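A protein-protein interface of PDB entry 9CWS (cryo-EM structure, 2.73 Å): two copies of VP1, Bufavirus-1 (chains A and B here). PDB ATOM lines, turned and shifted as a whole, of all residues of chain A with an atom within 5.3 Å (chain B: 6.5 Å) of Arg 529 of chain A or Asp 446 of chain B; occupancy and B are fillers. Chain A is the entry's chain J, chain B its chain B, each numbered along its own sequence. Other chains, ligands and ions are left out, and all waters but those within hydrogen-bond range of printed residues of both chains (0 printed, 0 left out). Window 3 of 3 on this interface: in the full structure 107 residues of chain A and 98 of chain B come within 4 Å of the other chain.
No position is printed for both chains.
Of chain B, only Asp 446, Ile 447 and Asn 448 come within 4 Å of Arg 529 of chain A.
Asp 446 of chain B touches one residue of chain A.
Of the printed residues of chain A, Gly 449 of chain B touches Ile 516 (2.7 Å).
Printed residues of chain B within 4 Å of Ile 516 of chain A: Ile 447, Asn 448, Gly 449 and Met 459.
Of the printed residues of chain B, Asp 518 of chain A touches Asn 448.
Of the printed residues of chain A, Asn 448 of chain B touches Ile 516, Phe 517, Asp 518 and Arg 529.
N of Gly 449 of chain B is in hydrogen-bond range of O of Ile 516 of chain A (2.7 Å).
The side-chain amide nitrogen of Asn 448 of chain B is in hydrogen-bond range of the side-chain carboxylate of Asp 518 of chain A (3.3 Å).
Among the printed residues, merely in contact across the chains: Ile 516 of chain A with Asn 448 of chain B (3.0 Å), Arg 529 of chain A with Ile 447 of chain B (3.5 Å), Ile 516 of chain A with Met 459 of chain B (3.6 Å), Phe 517 of chain A with Asn 448 of chain B (3.6 Å), Arg 529 of chain A with Asn 448 of chain B (3.7 Å), Arg 529 of chain A with Asp 446 of chain B (3.7 Å) and Ile 516 of chain A with Ile 447 of chain B (3.8 Å).
Of the 10 printed residues of chain B, 5 touch a printed residue of chain A.
Hydrophobic or aromatic side chains of chain A within 4 Å of the printed part of chain B: Ile 516.
Among the printed residues, no Asp or Glu carboxylate lies within 4 Å of a Lys or Arg side-chain nitrogen of the other chain.
The backbone carbonyl oxygen of Asp 518 of chain A is in hydrogen-bond range of the backbone NH of Asp 523 of chain A, at 2.9 Å.
The backbone NH (N) of Phe 517 of chain A lies within hydrogen-bond range of the backbone carbonyl oxygen (O) of Asp 530 of chain A, at 3.1 Å.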
ATOM      1  N   ILE A 516       1.191 -28.252  30.425  1.00  0.00           N
ATOM      2  CA  ILE A 516      -0.016 -28.482  29.645  1.00  0.00           C
ATOM      3  C   ILE A 516       0.409 -28.300  28.200  1.00  0.00           C
ATOM      4  O   ILE A 516       0.999 -27.274  27.856  1.00  0.00           O
ATOM      5  CB  ILE A 516      -1.132 -27.505  30.029  1.00  0.00           C
ATOM      6  CG1 ILE A 516      -1.251 -27.393  31.549  1.00  0.00           C
ATOM      7  CG2 ILE A 516      -2.450 -27.957  29.454  1.00  0.00           C
ATOM      8  CD1 ILE A 516      -1.554 -28.664  32.237  1.00  0.00           C
ATOM      9  N   PHE A 517       0.171 -29.290  27.355  1.00  0.00           N
ATOM     10  CA  PHE A 517       0.709 -29.262  26.003  1.00  0.00           C
ATOM     11  C   PHE A 517      -0.257 -29.911  25.022  1.00  0.00           C
ATOM     12  O   PHE A 517      -1.272 -30.492  25.402  1.00  0.00           O
ATOM     13  CB  PHE A 517       2.084 -29.933  25.977  1.00  0.00           C
ATOM     14  CG  PHE A 517       2.102 -31.305  26.574  1.00  0.00           C
ATOM     15  CD1 PHE A 517       1.861 -32.417  25.802  1.00  0.00           C
ATOM     16  CD2 PHE A 517       2.363 -31.478  27.917  1.00  0.00           C
ATOM     17  CE1 PHE A 517       1.875 -33.666  26.356  1.00  0.00           C
ATOM     18  CE2 PHE A 517       2.375 -32.723  28.472  1.00  0.00           C
ATOM     19  CZ  PHE A 517       2.131 -33.820  27.690  1.00  0.00           C
ATOM     20  N   ASP A 518       0.089 -29.837  23.739  1.00  0.00           N
ATOM     21  CA  ASP A 518      -0.829 -30.251  22.686  1.00  0.00           C
ATOM     22  C   ASP A 518      -0.157 -31.103  21.619  1.00  0.00           C
ATOM     23  O   ASP A 518       0.983 -31.540  21.784  1.00  0.00           O
ATOM     24  CB  ASP A 518      -1.500 -29.039  22.038  1.00  0.00           C
ATOM     25  CG  ASP A 518      -0.517 -28.104  21.374  1.00  0.00           C
ATOM     26  OD1 ASP A 518       0.703 -28.283  21.540  1.00  0.00           O
ATOM     27  OD2 ASP A 518      -0.971 -27.185  20.667  1.00  0.00           O
ATOM     28  N   ASP A 523       1.666 -34.272  22.643  1.00  0.00           N
ATOM     29  CA  ASP A 523       0.415 -34.932  22.983  1.00  0.00           C
ATOM     30  C   ASP A 523       0.033 -35.862  21.844  1.00  0.00           C
ATOM     31  O   ASP A 523       0.216 -35.520  20.674  1.00  0.00           O
ATOM     32  CB  ASP A 523      -0.684 -33.902  23.221  1.00  0.00           C
ATOM     33  CG  ASP A 523      -1.976 -34.516  23.664  1.00  0.00           C
ATOM     34  OD1 ASP A 523      -2.012 -35.727  23.936  1.00  0.00           O
ATOM     35  OD2 ASP A 523      -2.972 -33.785  23.723  1.00  0.00           O
ATOM     36  N   ALA A 527      -7.436 -32.044  19.586  1.00  0.00           N
ATOM     37  CA  ALA A 527      -8.705 -31.691  20.217  1.00  0.00           C
ATOM     38  C   ALA A 527      -8.662 -31.782  21.741  1.00  0.00           C
ATOM     39  O   ALA A 527      -9.615 -31.366  22.408  1.00  0.00           O
ATOM     40  CB  ALA A 527      -9.837 -32.568  19.673  1.00  0.00           C
ATOM     41  N   HIS A 528      -7.581 -32.313  22.307  1.00  0.00           N
ATOM     42  CA  HIS A 528      -7.405 -32.370  23.750  1.00  0.00           C
ATOM     43  C   HIS A 528      -5.944 -32.130  24.085  1.00  0.00           C
ATOM     44  O   HIS A 528      -5.069 -32.274  23.233  1.00  0.00           O
ATOM     45  CB  HIS A 528      -7.866 -33.707  24.334  1.00  0.00           C
ATOM     46  CG  HIS A 528      -9.337 -33.940  24.211  1.00  0.00           C
ATOM     47  ND1 HIS A 528      -9.913 -34.501  23.092  1.00  0.00           N
ATOM     48  CD2 HIS A 528     -10.356 -33.664  25.059  1.00  0.00           C
ATOM     49  CE1 HIS A 528     -11.221 -34.576  23.263  1.00  0.00           C
ATOM     50  NE2 HIS A 528     -11.515 -34.073  24.447  1.00  0.00           N
ATOM     51  N   ARG A 529      -5.692 -31.744  25.332  1.00  0.00           N
ATOM     52  CA  ARG A 529      -4.352 -31.434  25.809  1.00  0.00           C
ATOM     53  C   ARG A 529      -3.965 -32.354  26.953  1.00  0.00           C
ATOM     54  O   ARG A 529      -4.714 -32.495  27.924  1.00  0.00           O
ATOM     55  CB  ARG A 529      -4.247 -29.979  26.252  1.00  0.00           C
ATOM     56  CG  ARG A 529      -4.177 -29.025  25.108  1.00  0.00           C
ATOM     57  CD  ARG A 529      -4.040 -27.607  25.565  1.00  0.00           C
ATOM     58  NE  ARG A 529      -3.837 -26.720  24.428  1.00  0.00           N
ATOM     59  CZ  ARG A 529      -4.816 -26.245  23.671  1.00  0.00           C
ATOM     60  NH1 ARG A 529      -6.072 -26.567  23.926  1.00  0.00           N
ATOM     61  NH2 ARG A 529      -4.534 -25.445  22.658  1.00  0.00           N
ATOM     62  N   ASP A 530      -2.817 -33.000  26.812  1.00  0.00           N
ATOM     63  CA  ASP A 530      -2.241 -33.842  27.841  1.00  0.00           C
ATOM     64  C   ASP A 530      -1.476 -32.993  28.858  1.00  0.00           C
ATOM     65  O   ASP A 530      -1.142 -31.836  28.609  1.00  0.00           O
ATOM     66  CB  ASP A 530      -1.349 -34.907  27.214  1.00  0.00           C
ATOM     67  CG  ASP A 530      -1.162 -36.097  28.111  1.00  0.00           C
ATOM     68  OD1 ASP A 530      -1.762 -36.116  29.203  1.00  0.00           O
ATOM     69  OD2 ASP A 530      -0.445 -37.033  27.713  1.00  0.00           O
ATOM     70  N   GLN A 531      -1.241 -33.578  30.030  1.00  0.00           N
ATOM     71  CA  GLN A 531      -0.621 -32.908  31.164  1.00  0.00           C
ATOM     72  C   GLN A 531       0.544 -33.746  31.670  1.00  0.00           C
ATOM     73  O   GLN A 531       0.643 -34.934  31.364  1.00  0.00           O
ATOM     74  CB  GLN A 531      -1.628 -32.734  32.286  1.00  0.00           C
ATOM     75  CG  GLN A 531      -2.846 -31.999  31.866  1.00  0.00           C
ATOM     76  CD  GLN A 531      -3.934 -32.113  32.876  1.00  0.00           C
ATOM     77  OE1 GLN A 531      -3.926 -33.012  33.714  1.00  0.00           O
ATOM     78  NE2 GLN A 531      -4.920 -31.242  32.775  1.00  0.00           N
ATOM     79  N   PRO B 430      -2.403 -15.889  26.371  1.00  0.00           N
ATOM     80  CA  PRO B 430      -3.119 -15.878  25.091  1.00  0.00           C
ATOM     81  C   PRO B 430      -4.485 -15.225  25.198  1.00  0.00           C
ATOM     82  O   PRO B 430      -5.292 -15.578  26.058  1.00  0.00           O
ATOM     83  CB  PRO B 430      -3.218 -17.364  24.746  1.00  0.00           C
ATOM     84  CG  PRO B 430      -2.032 -17.951  25.394  1.00  0.00           C
ATOM     85  CD  PRO B 430      -1.862 -17.222  26.676  1.00  0.00           C
ATOM     86  N   ASN B 443      -9.352 -13.571  27.607  1.00  0.00           N
ATOM     87  CA  ASN B 443      -8.340 -14.591  27.838  1.00  0.00           C
ATOM     88  C   ASN B 443      -8.834 -15.934  27.325  1.00  0.00           C
ATOM     89  O   ASN B 443      -9.959 -16.344  27.621  1.00  0.00           O
ATOM     90  CB  ASN B 443      -8.008 -14.674  29.326  1.00  0.00           C
ATOM     91  CG  ASN B 443      -7.279 -13.457  29.828  1.00  0.00           C
ATOM     92  OD1 ASN B 443      -6.099 -13.278  29.565  1.00  0.00           O
ATOM     93  ND2 ASN B 443      -7.976 -12.617  30.567  1.00  0.00           N
ATOM     94  N   ILE B 444      -7.992 -16.604  26.535  1.00  0.00           N
ATOM     95  CA  ILE B 444      -8.370 -17.932  25.972  1.00  0.00           C
ATOM     96  C   ILE B 444      -8.383 -18.950  27.114  1.00  0.00           C
ATOM     97  O   ILE B 444      -7.411 -18.978  27.890  1.00  0.00           O
ATOM     98  CB  ILE B 444      -7.423 -18.335  24.825  1.00  0.00           C
ATOM     99  CG1 ILE B 444      -7.392 -17.268  23.728  1.00  0.00           C
ATOM    100  CG2 ILE B 444      -7.794 -19.704  24.274  1.00  0.00           C
ATOM    101  CD1 ILE B 444      -6.363 -17.519  22.652  1.00  0.00           C
ATOM    102  N   ARG B 445      -9.453 -19.740  27.213  1.00  0.00           N
ATOM    103  CA  ARG B 445      -9.594 -20.713  28.290  1.00  0.00           C
ATOM    104  C   ARG B 445      -8.712 -21.936  28.067  1.00  0.00           C
ATOM    105  O   ARG B 445      -7.970 -22.350  28.963  1.00  0.00           O
ATOM    106  CB  ARG B 445     -11.059 -21.114  28.444  1.00  0.00           C
ATOM    107  CG  ARG B 445     -11.937 -19.975  28.907  1.00  0.00           C
ATOM    108  CD  ARG B 445     -13.367 -20.420  29.101  1.00  0.00           C
ATOM    109  NE  ARG B 445     -14.227 -19.320  29.529  1.00  0.00           N
ATOM    110  CZ  ARG B 445     -15.543 -19.421  29.691  1.00  0.00           C
ATOM    111  NH1 ARG B 445     -16.156 -20.575  29.464  1.00  0.00           N
ATOM    112  NH2 ARG B 445     -16.246 -18.368  30.084  1.00  0.00           N
ATOM    113  N   ASP B 446      -8.766 -22.528  26.874  1.00  0.00           N
ATOM    114  CA  ASP B 446      -7.953 -23.708  26.585  1.00  0.00           C
ATOM    115  C   ASP B 446      -6.655 -23.262  25.928  1.00  0.00           C
ATOM    116  O   ASP B 446      -6.599 -22.886  24.756  1.00  0.00           O
ATOM    117  CB  ASP B 446      -8.708 -24.690  25.699  1.00  0.00           C
ATOM    118  CG  ASP B 446      -9.795 -25.431  26.443  1.00  0.00           C
ATOM    119  OD1 ASP B 446      -9.753 -25.466  27.690  1.00  0.00           O
ATOM    120  OD2 ASP B 446     -10.698 -25.981  25.782  1.00  0.00           O
ATOM    121  N   ILE B 447      -5.582 -23.350  26.700  1.00  0.00           N
ATOM    122  CA  ILE B 447      -4.242 -23.030  26.246  1.00  0.00           C
ATOM    123  C   ILE B 447      -3.304 -24.060  26.846  1.00  0.00           C
ATOM    124  O   ILE B 447      -3.670 -24.835  27.732  1.00  0.00           O
ATOM    125  CB  ILE B 447      -3.792 -21.606  26.634  1.00  0.00           C
ATOM    126  CG1 ILE B 447      -3.787 -21.446  28.148  1.00  0.00           C
ATOM    127  CG2 ILE B 447      -4.676 -20.553  26.000  1.00  0.00           C
ATOM    128  CD1 ILE B 447      -3.114 -20.214  28.601  1.00  0.00           C
ATOM    129  N   ASN B 448      -2.078 -24.070  26.348  1.00  0.00           N
ATOM    130  CA  ASN B 448      -1.036 -24.948  26.849  1.00  0.00           C
ATOM    131  C   ASN B 448       0.072 -24.093  27.442  1.00  0.00           C
ATOM    132  O   ASN B 448       0.200 -22.922  27.086  1.00  0.00           O
ATOM    133  CB  ASN B 448      -0.529 -25.871  25.731  1.00  0.00           C
ATOM    134  CG  ASN B 448      -0.009 -25.124  24.539  1.00  0.00           C
ATOM    135  OD1 ASN B 448      -0.253 -23.935  24.383  1.00  0.00           O
ATOM    136  ND2 ASN B 448       0.708 -25.823  23.679  1.00  0.00           N
ATOM    137  N   GLY B 449       0.829 -24.652  28.377  1.00  0.00           N
ATOM    138  CA  GLY B 449       1.881 -23.890  29.016  1.00  0.00           C
ATOM    139  C   GLY B 449       2.326 -24.529  30.308  1.00  0.00           C
ATOM    140  O   GLY B 449       1.949 -25.651  30.631  1.00  0.00           O
ATOM    141  N   ASP B 457      -6.252 -26.854  35.020  1.00  0.00           N
ATOM    142  CA  ASP B 457      -7.399 -26.273  34.329  1.00  0.00           C
ATOM    143  C   ASP B 457      -7.398 -24.751  34.371  1.00  0.00           C
ATOM    144  O   ASP B 457      -7.511 -24.115  33.315  1.00  0.00           O
ATOM    145  CB  ASP B 457      -8.712 -26.811  34.895  1.00  0.00           C
ATOM    146  CG  ASP B 457      -9.915 -26.158  34.274  1.00  0.00           C
ATOM    147  OD1 ASP B 457     -10.157 -26.375  33.072  1.00  0.00           O
ATOM    148  OD2 ASP B 457     -10.615 -25.410  34.982  1.00  0.00           O
ATOM    149  N   MET B 459      -5.664 -21.985  33.797  1.00  0.00           N
ATOM    150  CA  MET B 459      -4.400 -21.653  33.154  1.00  0.00           C
ATOM    151  C   MET B 459      -4.036 -20.189  33.372  1.00  0.00           C
ATOM    152  O   MET B 459      -3.226 -19.629  32.633  1.00  0.00           O
ATOM    153  CB  MET B 459      -4.441 -21.974  31.663  1.00  0.00           C
ATOM    154  CG  MET B 459      -4.435 -23.454  31.342  1.00  0.00           C
ATOM    155  SD  MET B 459      -2.944 -24.279  31.899  1.00  0.00           S
ATOM    156  CE  MET B 459      -1.720 -23.532  30.848  1.00  0.00           C
